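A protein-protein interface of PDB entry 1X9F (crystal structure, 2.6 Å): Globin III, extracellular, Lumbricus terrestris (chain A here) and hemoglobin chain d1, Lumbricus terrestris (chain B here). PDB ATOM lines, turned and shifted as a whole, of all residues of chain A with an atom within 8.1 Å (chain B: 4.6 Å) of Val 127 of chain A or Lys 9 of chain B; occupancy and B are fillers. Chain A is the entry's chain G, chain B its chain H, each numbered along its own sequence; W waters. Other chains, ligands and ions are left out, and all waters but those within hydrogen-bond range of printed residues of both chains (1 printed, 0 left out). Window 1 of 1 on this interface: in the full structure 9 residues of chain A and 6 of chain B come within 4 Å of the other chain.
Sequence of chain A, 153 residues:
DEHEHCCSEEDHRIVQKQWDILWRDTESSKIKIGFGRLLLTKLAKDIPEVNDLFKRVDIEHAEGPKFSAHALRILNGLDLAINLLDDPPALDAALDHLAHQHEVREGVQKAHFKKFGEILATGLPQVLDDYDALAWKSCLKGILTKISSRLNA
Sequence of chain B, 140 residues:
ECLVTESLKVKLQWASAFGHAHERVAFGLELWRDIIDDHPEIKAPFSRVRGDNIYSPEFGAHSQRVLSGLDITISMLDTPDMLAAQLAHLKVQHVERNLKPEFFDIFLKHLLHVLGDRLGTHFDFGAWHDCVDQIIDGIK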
ATOM      1  N   GLN A  18       0.856  17.673 -25.689  1.00  0.00           N
ATOM      2  CA  GLN A  18       1.261  16.683 -24.697  1.00  0.00           C
ATOM      3  C   GLN A  18       0.420  15.426 -24.768  1.00  0.00           C
ATOM      4  O   GLN A  18       0.929  14.315 -24.594  1.00  0.00           O
ATOM      5  CB  GLN A  18       1.237  17.291 -23.299  1.00  0.00           C
ATOM      6  CG  GLN A  18       2.284  18.375 -23.163  1.00  0.00           C
ATOM      7  CD  GLN A  18       2.282  19.066 -21.818  1.00  0.00           C
ATOM      8  OE1 GLN A  18       3.285  19.674 -21.443  1.00  0.00           O
ATOM      9  NE2 GLN A  18       1.172  18.991 -21.093  1.00  0.00           N
ATOM     10  N   TRP A  19      -0.868  15.613 -25.044  1.00  0.00           N
ATOM     11  CA  TRP A  19      -1.805  14.512 -25.226  1.00  0.00           C
ATOM     12  C   TRP A  19      -1.490  13.687 -26.474  1.00  0.00           C
ATOM     13  O   TRP A  19      -1.395  12.462 -26.387  1.00  0.00           O
ATOM     14  CB  TRP A  19      -3.221  15.070 -25.281  1.00  0.00           C
ATOM     15  CG  TRP A  19      -4.321  14.098 -25.545  1.00  0.00           C
ATOM     16  CD1 TRP A  19      -5.020  13.958 -26.708  1.00  0.00           C
ATOM     17  CD2 TRP A  19      -4.894  13.171 -24.618  1.00  0.00           C
ATOM     18  NE1 TRP A  19      -5.991  12.992 -26.567  1.00  0.00           N
ATOM     19  CE2 TRP A  19      -5.937  12.494 -25.293  1.00  0.00           C
ATOM     20  CE3 TRP A  19      -4.634  12.838 -23.280  1.00  0.00           C
ATOM     21  CZ2 TRP A  19      -6.708  11.502 -24.682  1.00  0.00           C
ATOM     22  CZ3 TRP A  19      -5.403  11.852 -22.672  1.00  0.00           C
ATOM     23  CH2 TRP A  19      -6.425  11.196 -23.375  1.00  0.00           C
ATOM     24  N   ILE A  21       1.052  12.857 -27.795  1.00  0.00           N
ATOM     25  CA  ILE A  21       2.182  11.969 -27.564  1.00  0.00           C
ATOM     26  C   ILE A  21       1.765  10.538 -27.230  1.00  0.00           C
ATOM     27  O   ILE A  21       2.456   9.593 -27.604  1.00  0.00           O
ATOM     28  CB  ILE A  21       3.109  12.578 -26.487  1.00  0.00           C
ATOM     29  CG1 ILE A  21       4.052  13.598 -27.141  1.00  0.00           C
ATOM     30  CG2 ILE A  21       3.909  11.499 -25.748  1.00  0.00           C
ATOM     31  CD1 ILE A  21       4.548  14.692 -26.208  1.00  0.00           C
ATOM     32  N   LEU A  22       0.630  10.373 -26.554  1.00  0.00           N
ATOM     33  CA  LEU A  22       0.142   9.033 -26.226  1.00  0.00           C
ATOM     34  C   LEU A  22      -0.224   8.155 -27.434  1.00  0.00           C
ATOM     35  O   LEU A  22      -0.386   6.940 -27.275  1.00  0.00           O
ATOM     36  CB  LEU A  22      -1.052   9.101 -25.264  1.00  0.00           C
ATOM     37  CG  LEU A  22      -0.807   9.301 -23.767  1.00  0.00           C
ATOM     38  CD1 LEU A  22      -2.137   9.364 -23.029  1.00  0.00           C
ATOM     39  CD2 LEU A  22       0.075   8.205 -23.177  1.00  0.00           C
ATOM     40  N   TRP A  23      -0.361   8.739 -28.627  1.00  0.00           N
ATOM     41  CA  TRP A  23      -0.804   7.949 -29.791  1.00  0.00           C
ATOM     42  C   TRP A  23       0.237   7.905 -30.897  1.00  0.00           C
ATOM     43  O   TRP A  23      -0.086   7.620 -32.054  1.00  0.00           O
ATOM     44  CB  TRP A  23      -2.162   8.442 -30.313  1.00  0.00           C
ATOM     45  CG  TRP A  23      -2.935   9.102 -29.238  1.00  0.00           C
ATOM     46  CD1 TRP A  23      -3.139  10.442 -29.086  1.00  0.00           C
ATOM     47  CD2 TRP A  23      -3.547   8.473 -28.108  1.00  0.00           C
ATOM     48  NE1 TRP A  23      -3.862  10.687 -27.943  1.00  0.00           N
ATOM     49  CE2 TRP A  23      -4.122   9.496 -27.318  1.00  0.00           C
ATOM     50  CE3 TRP A  23      -3.676   7.144 -27.679  1.00  0.00           C
ATOM     51  CZ2 TRP A  23      -4.821   9.236 -26.138  1.00  0.00           C
ATOM     52  CZ3 TRP A  23      -4.370   6.886 -26.502  1.00  0.00           C
ATOM     53  CH2 TRP A  23      -4.935   7.930 -25.747  1.00  0.00           C
ATOM     54  N   ILE A  31      -3.730   1.232 -25.247  1.00  0.00           N
ATOM     55  CA  ILE A  31      -3.417   2.338 -24.345  1.00  0.00           C
ATOM     56  C   ILE A  31      -4.685   2.985 -23.803  1.00  0.00           C
ATOM     57  O   ILE A  31      -4.787   3.257 -22.605  1.00  0.00           O
ATOM     58  CB  ILE A  31      -2.545   3.394 -25.068  1.00  0.00           C
ATOM     59  CG1 ILE A  31      -1.186   2.795 -25.443  1.00  0.00           C
ATOM     60  CG2 ILE A  31      -2.370   4.643 -24.199  1.00  0.00           C
ATOM     61  CD1 ILE A  31      -0.322   3.692 -26.308  1.00  0.00           C
ATOM     62  N   GLY A  34      -6.410   0.384 -21.278  1.00  0.00           N
ATOM     63  CA  GLY A  34      -5.625   0.275 -20.057  1.00  0.00           C
ATOM     64  C   GLY A  34      -5.800   1.509 -19.200  1.00  0.00           C
ATOM     65  O   GLY A  34      -6.103   1.413 -18.009  1.00  0.00           O
ATOM     66  N   PHE A  35      -5.636   2.672 -19.820  1.00  0.00           N
ATOM     67  CA  PHE A  35      -5.712   3.926 -19.091  1.00  0.00           C
ATOM     68  C   PHE A  35      -7.134   4.252 -18.602  1.00  0.00           C
ATOM     69  O   PHE A  35      -7.323   4.561 -17.425  1.00  0.00           O
ATOM     70  CB  PHE A  35      -5.100   5.063 -19.918  1.00  0.00           C
ATOM     71  CG  PHE A  35      -4.865   6.327 -19.139  1.00  0.00           C
ATOM     72  CD1 PHE A  35      -4.115   6.319 -17.963  1.00  0.00           C
ATOM     73  CD2 PHE A  35      -5.380   7.536 -19.592  1.00  0.00           C
ATOM     74  CE1 PHE A  35      -3.895   7.499 -17.245  1.00  0.00           C
ATOM     75  CE2 PHE A  35      -5.165   8.721 -18.883  1.00  0.00           C
ATOM     76  CZ  PHE A  35      -4.420   8.702 -17.707  1.00  0.00           C
ATOM     77  N   LEU A  38      -8.127   1.938 -15.889  1.00  0.00           N
ATOM     78  CA  LEU A  38      -7.453   2.319 -14.654  1.00  0.00           C
ATOM     79  C   LEU A  38      -8.177   3.473 -13.959  1.00  0.00           C
ATOM     80  O   LEU A  38      -8.411   3.424 -12.751  1.00  0.00           O
ATOM     81  CB  LEU A  38      -5.996   2.702 -14.932  1.00  0.00           C
ATOM     82  CG  LEU A  38      -5.265   3.361 -13.760  1.00  0.00           C
ATOM     83  CD1 LEU A  38      -4.174   2.450 -13.208  1.00  0.00           C
ATOM     84  CD2 LEU A  38      -4.686   4.693 -14.197  1.00  0.00           C
ATOM     85  N   LEU A 120      -7.577  12.015 -12.577  1.00  0.00           N
ATOM     86  CA  LEU A 120      -7.051  12.300 -13.901  1.00  0.00           C
ATOM     87  C   LEU A 120      -5.780  13.142 -13.846  1.00  0.00           C
ATOM     88  O   LEU A 120      -4.835  12.873 -14.588  1.00  0.00           O
ATOM     89  CB  LEU A 120      -8.124  12.979 -14.761  1.00  0.00           C
ATOM     90  CG  LEU A 120      -7.971  13.095 -16.282  1.00  0.00           C
ATOM     91  CD1 LEU A 120      -7.441  11.818 -16.909  1.00  0.00           C
ATOM     92  CD2 LEU A 120      -9.299  13.478 -16.916  1.00  0.00           C
ATOM     93  N   THR A 122      -3.666  13.189 -11.446  1.00  0.00           N
ATOM     94  CA  THR A 122      -2.621  12.343 -10.894  1.00  0.00           C
ATOM     95  C   THR A 122      -2.084  11.369 -11.935  1.00  0.00           C
ATOM     96  O   THR A 122      -0.868  11.190 -12.047  1.00  0.00           O
ATOM     97  CB  THR A 122      -3.142  11.588  -9.650  1.00  0.00           C
ATOM     98  OG1 THR A 122      -3.217  12.496  -8.545  1.00  0.00           O
ATOM     99  CG2 THR A 122      -2.131  10.543  -9.165  1.00  0.00           C
ATOM    100  N   GLY A 123      -2.986  10.747 -12.693  1.00  0.00           N
ATOM    101  CA  GLY A 123      -2.619   9.683 -13.625  1.00  0.00           C
ATOM    102  C   GLY A 123      -1.939  10.135 -14.908  1.00  0.00           C
ATOM    103  O   GLY A 123      -1.119   9.400 -15.465  1.00  0.00           O
ATOM    104  N   LEU A 124      -2.267  11.327 -15.395  1.00  0.00           N
ATOM    105  CA  LEU A 124      -1.699  11.783 -16.669  1.00  0.00           C
ATOM    106  C   LEU A 124      -0.175  11.907 -16.662  1.00  0.00           C
ATOM    107  O   LEU A 124       0.483  11.421 -17.589  1.00  0.00           O
ATOM    108  CB  LEU A 124      -2.349  13.085 -17.138  1.00  0.00           C
ATOM    109  CG  LEU A 124      -3.733  12.916 -17.760  1.00  0.00           C
ATOM    110  CD1 LEU A 124      -4.462  14.245 -17.757  1.00  0.00           C
ATOM    111  CD2 LEU A 124      -3.648  12.332 -19.176  1.00  0.00           C
ATOM    112  N   PRO A 125       0.393  12.567 -15.650  1.00  0.00           N
ATOM    113  CA  PRO A 125       1.843  12.651 -15.529  1.00  0.00           C
ATOM    114  C   PRO A 125       2.522  11.296 -15.370  1.00  0.00           C
ATOM    115  O   PRO A 125       3.700  11.164 -15.701  1.00  0.00           O
ATOM    116  CB  PRO A 125       2.055  13.501 -14.270  1.00  0.00           C
ATOM    117  CG  PRO A 125       0.781  13.474 -13.548  1.00  0.00           C
ATOM    118  CD  PRO A 125      -0.280  13.324 -14.579  1.00  0.00           C
ATOM    119  N   GLN A 126       1.799  10.300 -14.871  1.00  0.00           N
ATOM    120  CA  GLN A 126       2.371   8.965 -14.757  1.00  0.00           C
ATOM    121  C   GLN A 126       2.538   8.290 -16.113  1.00  0.00           C
ATOM    122  O   GLN A 126       3.240   7.281 -16.218  1.00  0.00           O
ATOM    123  CB  GLN A 126       1.512   8.091 -13.857  1.00  0.00           C
ATOM    124  CG  GLN A 126       1.510   8.534 -12.420  1.00  0.00           C
ATOM    125  CD  GLN A 126       0.551   7.736 -11.578  1.00  0.00           C
ATOM    126  OE1 GLN A 126       0.425   7.988 -10.382  1.00  0.00           O
ATOM    127  NE2 GLN A 126      -0.134   6.773 -12.190  1.00  0.00           N
ATOM    128  N   VAL A 127       1.896   8.837 -17.146  1.00  0.00           N
ATOM    129  CA  VAL A 127       2.027   8.275 -18.495  1.00  0.00           C
ATOM    130  C   VAL A 127       2.670   9.230 -19.500  1.00  0.00           C
ATOM    131  O   VAL A 127       3.291   8.791 -20.470  1.00  0.00           O
ATOM    132  CB  VAL A 127       0.682   7.725 -19.059  1.00  0.00           C
ATOM    133  CG1 VAL A 127       0.090   6.681 -18.132  1.00  0.00           C
ATOM    134  CG2 VAL A 127      -0.323   8.837 -19.327  1.00  0.00           C
ATOM    135  N   LEU A 128       2.503  10.529 -19.274  1.00  0.00           N
ATOM    136  CA  LEU A 128       3.095  11.546 -20.131  1.00  0.00           C
ATOM    137  C   LEU A 128       4.295  12.095 -19.391  1.00  0.00           C
ATOM    138  O   LEU A 128       4.174  12.531 -18.243  1.00  0.00           O
ATOM    139  CB  LEU A 128       2.103  12.683 -20.394  1.00  0.00           C
ATOM    140  CG  LEU A 128       0.697  12.370 -20.919  1.00  0.00           C
ATOM    141  CD1 LEU A 128      -0.169  13.625 -20.894  1.00  0.00           C
ATOM    142  CD2 LEU A 128       0.812  11.827 -22.333  1.00  0.00           C
ATOM    143  N   ASP A 129       5.457  12.075 -20.028  1.00  0.00           N
ATOM    144  CA  ASP A 129       6.650  12.578 -19.357  1.00  0.00           C
ATOM    145  C   ASP A 129       6.856  14.071 -19.591  1.00  0.00           C
ATOM    146  O   ASP A 129       7.876  14.642 -19.200  1.00  0.00           O
ATOM    147  CB  ASP A 129       7.881  11.790 -19.780  1.00  0.00           C
ATOM    148  CG  ASP A 129       8.219  11.968 -21.245  1.00  0.00           C
ATOM    149  OD1 ASP A 129       7.575  12.783 -21.947  1.00  0.00           O
ATOM    150  OD2 ASP A 129       9.137  11.316 -21.783  1.00  0.00           O
ATOM    151  N   ASP A 130       5.882  14.687 -20.248  1.00  0.00           N
ATOM    152  CA  ASP A 130       5.870  16.119 -20.469  1.00  0.00           C
ATOM    153  C   ASP A 130       4.474  16.607 -20.109  1.00  0.00           C
ATOM    154  O   ASP A 130       3.515  16.330 -20.829  1.00  0.00           O
ATOM    155  CB  ASP A 130       6.189  16.414 -21.933  1.00  0.00           C
ATOM    156  CG  ASP A 130       6.509  17.868 -22.178  1.00  0.00           C
ATOM    157  OD1 ASP A 130       6.287  18.336 -23.315  1.00  0.00           O
ATOM    158  OD2 ASP A 130       6.985  18.623 -21.304  1.00  0.00           O
ATOM    159  N   TYR A 131       4.353  17.316 -18.991  1.00  0.00           N
ATOM    160  CA  TYR A 131       3.038  17.606 -18.434  1.00  0.00           C
ATOM    161  C   TYR A 131       2.968  18.948 -17.729  1.00  0.00           C
ATOM    162  O   TYR A 131       3.493  19.102 -16.624  1.00  0.00           O
ATOM    163  CB  TYR A 131       2.648  16.496 -17.453  1.00  0.00           C
ATOM    164  CG  TYR A 131       1.281  16.675 -16.847  1.00  0.00           C
ATOM    165  CD1 TYR A 131       0.131  16.398 -17.585  1.00  0.00           C
ATOM    166  CD2 TYR A 131       1.133  17.105 -15.528  1.00  0.00           C
ATOM    167  CE1 TYR A 131      -1.134  16.553 -17.028  1.00  0.00           C
ATOM    168  CE2 TYR A 131      -0.127  17.263 -14.962  1.00  0.00           C
ATOM    169  CZ  TYR A 131      -1.255  16.990 -15.719  1.00  0.00           C
ATOM    170  OH  TYR A 131      -2.504  17.147 -15.164  1.00  0.00           O
ATOM    171  N   THR B   5       0.214   2.260 -15.682  1.00  0.00           N
ATOM    172  CA  THR B   5       0.769   3.551 -16.086  1.00  0.00           C
ATOM    173  C   THR B   5       2.291   3.512 -16.198  1.00  0.00           C
ATOM    174  O   THR B   5       2.870   4.118 -17.105  1.00  0.00           O
ATOM    175  CB  THR B   5       0.321   4.677 -15.137  1.00  0.00           C
ATOM    176  OG1 THR B   5       0.688   4.349 -13.792  1.00  0.00           O
ATOM    177  CG2 THR B   5      -1.195   4.768 -15.083  1.00  0.00           C
ATOM    178  N   GLU B   6       2.927   2.787 -15.286  1.00  0.00           N
ATOM    179  CA  GLU B   6       4.380   2.687 -15.268  1.00  0.00           C
ATOM    180  C   GLU B   6       4.919   1.885 -16.449  1.00  0.00           C
ATOM    181  O   GLU B   6       5.917   2.270 -17.063  1.00  0.00           O
ATOM    182  CB  GLU B   6       4.848   2.073 -13.955  1.00  0.00           C
ATOM    183  CG  GLU B   6       4.385   2.826 -12.713  1.00  0.00           C
ATOM    184  CD  GLU B   6       4.982   2.239 -11.450  1.00  0.00           C
ATOM    185  OE1 GLU B   6       5.400   3.020 -10.567  1.00  0.00           O
ATOM    186  OE2 GLU B   6       5.048   0.993 -11.340  1.00  0.00           O
ATOM    187  N   SER B   7       4.264   0.774 -16.762  1.00  0.00           N
ATOM    188  CA  SER B   7       4.650  -0.015 -17.917  1.00  0.00           C
ATOM    189  C   SER B   7       4.481   0.827 -19.162  1.00  0.00           C
ATOM    190  O   SER B   7       5.298   0.756 -20.082  1.00  0.00           O
ATOM    191  CB  SER B   7       3.787  -1.268 -18.022  1.00  0.00           C
ATOM    192  OG  SER B   7       2.441  -0.932 -18.309  1.00  0.00           O
ATOM    193  N   LEU B   8       3.422   1.627 -19.179  1.00  0.00           N
ATOM    194  CA  LEU B   8       3.135   2.460 -20.329  1.00  0.00           C
ATOM    195  C   LEU B   8       4.200   3.555 -20.473  1.00  0.00           C
ATOM    196  O   LEU B   8       4.690   3.819 -21.579  1.00  0.00           O
ATOM    197  CB  LEU B   8       1.713   3.024 -20.223  1.00  0.00           C
ATOM    198  CG  LEU B   8       1.058   3.709 -21.424  1.00  0.00           C
ATOM    199  CD1 LEU B   8       1.239   5.206 -21.358  1.00  0.00           C
ATOM    200  CD2 LEU B   8       1.499   3.158 -22.779  1.00  0.00           C
ATOM    201  N   LYS B   9       4.558   4.159 -19.340  1.00  0.00           N
ATOM    202  CA  LYS B   9       5.630   5.144 -19.264  1.00  0.00           C
ATOM    203  C   LYS B   9       6.960   4.583 -19.759  1.00  0.00           C
ATOM    204  O   LYS B   9       7.660   5.239 -20.537  1.00  0.00           O
ATOM    205  CB  LYS B   9       5.776   5.646 -17.823  1.00  0.00           C
ATOM    206  CG  LYS B   9       6.724   6.827 -17.647  1.00  0.00           C
ATOM    207  CD  LYS B   9       6.209   8.064 -18.364  1.00  0.00           C
ATOM    208  CE  LYS B   9       6.487   9.333 -17.570  1.00  0.00           C
ATOM    209  NZ  LYS B   9       5.687   9.426 -16.319  1.00  0.00           N
ATOM    210  N   VAL B  10       7.296   3.373 -19.311  1.00  0.00           N
ATOM    211  CA  VAL B  10       8.555   2.735 -19.686  1.00  0.00           C
ATOM    212  C   VAL B  10       8.589   2.457 -21.188  1.00  0.00           C
ATOM    213  O   VAL B  10       9.600   2.707 -21.842  1.00  0.00           O
ATOM    214  CB  VAL B  10       8.829   1.457 -18.846  1.00  0.00           C
ATOM    215  CG1 VAL B  10       9.919   0.598 -19.468  1.00  0.00           C
ATOM    216  CG2 VAL B  10       9.199   1.829 -17.417  1.00  0.00           C
ATOM    217  N   LYS B  11       7.479   1.970 -21.735  1.00  0.00           N
ATOM    218  CA  LYS B  11       7.390   1.725 -23.172  1.00  0.00           C
ATOM    219  C   LYS B  11       7.646   3.010 -23.938  1.00  0.00           C
ATOM    220  O   LYS B  11       8.475   3.040 -24.851  1.00  0.00           O
ATOM    221  CB  LYS B  11       6.013   1.191 -23.554  1.00  0.00           C
ATOM    222  CG  LYS B  11       5.708  -0.217 -23.085  1.00  0.00           C
ATOM    223  CD  LYS B  11       4.231  -0.523 -23.306  1.00  0.00           C
ATOM    224  CE  LYS B  11       3.837  -1.877 -22.730  1.00  0.00           C
ATOM    225  NZ  LYS B  11       4.396  -3.020 -23.519  1.00  0.00           N
ATOM    226  N   LEU B  12       6.932   4.070 -23.564  1.00  0.00           N
ATOM    227  CA  LEU B  12       7.046   5.347 -24.260  1.00  0.00           C
ATOM    228  C   LEU B  12       8.456   5.905 -24.156  1.00  0.00           C
ATOM    229  O   LEU B  12       9.037   6.325 -25.158  1.00  0.00           O
ATOM    230  CB  LEU B  12       6.018   6.357 -23.732  1.00  0.00           C
ATOM    231  CG  LEU B  12       4.620   6.444 -24.369  1.00  0.00           C
ATOM    232  CD1 LEU B  12       4.164   5.180 -25.108  1.00  0.00           C
ATOM    233  CD2 LEU B  12       3.592   6.866 -23.324  1.00  0.00           C
ATOM    234  N   GLN B  13       9.013   5.891 -22.950  1.00  0.00           N
ATOM    235  CA  GLN B  13      10.345   6.429 -22.749  1.00  0.00           C
ATOM    236  C   GLN B  13      11.400   5.583 -23.438  1.00  0.00           C
ATOM    237  O   GLN B  13      12.373   6.119 -23.969  1.00  0.00           O
ATOM    238  CB  GLN B  13      10.653   6.607 -21.264  1.00  0.00           C
ATOM    239  CG  GLN B  13       9.774   7.658 -20.617  1.00  0.00           C
ATOM    240  CD  GLN B  13      10.378   8.256 -19.373  1.00  0.00           C
ATOM    241  OE1 GLN B  13      10.923   7.544 -18.528  1.00  0.00           O
ATOM    242  NE2 GLN B  13      10.278   9.573 -19.246  1.00  0.00           N
ATOM    243  N   ASP B 124      11.343   8.861 -15.893  1.00  0.00           N
ATOM    244  CA  ASP B 124      10.521   8.309 -14.829  1.00  0.00           C
ATOM    245  C   ASP B 124      11.271   7.184 -14.115  1.00  0.00           C
ATOM    246  O   ASP B 124      10.994   5.999 -14.312  1.00  0.00           O
ATOM    247  CB  ASP B 124       9.176   7.841 -15.375  1.00  0.00           C
ATOM    248  CG  ASP B 124       8.130   7.704 -14.296  1.00  0.00           C
ATOM    249  OD1 ASP B 124       6.926   7.801 -14.614  1.00  0.00           O
ATOM    250  OD2 ASP B 124       8.410   7.494 -13.094  1.00  0.00           O
ATOM    251  N   ALA B 127       9.141   4.562 -12.244  1.00  0.00           N
ATOM    252  CA  ALA B 127       8.556   3.586 -13.160  1.00  0.00           C
ATOM    253  C   ALA B 127       9.600   2.620 -13.695  1.00  0.00           C
ATOM    254  O   ALA B 127       9.423   1.410 -13.586  1.00  0.00           O
ATOM    255  CB  ALA B 127       7.832   4.283 -14.307  1.00  0.00           C
HETATM  256  O   HOH W   1       4.674   6.354 -13.666  1.00  0.00           O
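Of chain B, only Thr 5, Leu 8, Lys 9 and Leu 12 come within 4 Å of Val 127 of chain A. Lys 9 of chain B touches just these residues of chain A: Pro 125, Gln 126, Val 127, Leu 128 and Asp 129. Printed residues of chain B within 4 Å of Pro 125 of chain A: Lys 9 (2.7 Å). Printed residues of chain B within 4 Å of Ile 31 of chain A: Leu 8. Of the printed residues of chain B, Gln 126 of chain A touches Thr 5 (3.0 Å) and Lys 9 (3.3 Å). Printed residues of chain B within 4 Å of Leu 128 of chain A: Lys 9. Asp 124 of chain B touches none of the printed residues of chain A. Val 10 of chain B touches none of the printed residues of chain A. The nearest printed residue of chain B that does not touch Val 127 of chain A is Glu 6 of chain B (5.6 Å). The nearest residue of chain A that does not touch Lys 9 of chain B is Leu 124 of chain A (5.7 Å). The nearest printed residue of chain B that does not touch Leu 38 of chain A is Glu 6 of chain B (7.4 Å).
O of Pro 125 of chain A lies within hydrogen-bond range of NZ of Lys 9 of chain B (2.7 Å). NE2 of Gln 126 of chain A lies within hydrogen-bond range of OG1 of Thr 5 of chain B, at 3.0 Å. NZ of Lys 9 of chain B is in hydrogen-bond range of O of Gln 126 of chain A (3.3 Å). The side-chain carboxylate of Asp 129 of chain A is in hydrogen-bond range of the side-chain amide nitrogen of Gln 13 of chain B, 3.3 Å away.
Among the printed residues, merely in contact across the chains: Leu 22 of chain A with Leu 8 of chain B (3.7 Å), Leu 22 of chain A with Leu 12 of chain B (3.8 Å), Ile 31 of chain A with Leu 8 of chain B (3.8 Å), Leu 38 of chain A with Thr 5 of chain B (3.6 Å), Val 127 of chain A with Thr 5 of chain B (3.6 Å), Val 127 of chain A with Leu 8 of chain B (3.5 Å), Val 127 of chain A with Lys 9 of chain B (3.7 Å), Val 127 of chain A with Leu 12 of chain B (3.5 Å), Leu 128 of chain A with Lys 9 of chain B (3.95 Å) and Asp 129 of chain A with Lys 9 of chain B (3.6 Å).
Of the 20 printed residues of chain A, 8 touch a printed residue of chain B. Printed residues of chain A that touch a printed residue of chain B: Leu 22, Ile 31, Leu 38, Pro 125, Gln 126, Val 127, Leu 128 and Asp 129. Among the printed residues, no Asp or Glu carboxylate lies within 4 Å of a Lys or Arg side-chain nitrogen of the other chain.
The side-chain amino group (NZ) of Lys 9 of chain B lies within salt-bridge range of the side-chain carboxylate (OD1) of Asp 124 of chain B (2.7 Å). OE1 of Gln 13 of chain B is in hydrogen-bond range of N of Asp 124 of chain B (3.0 Å).
Water W1 bridges the side-chain carboxylate of Asp 124 of chain B (2.8 Å) and the backbone carbonyl oxygen of Gln 126 of chain A (3.1 Å).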
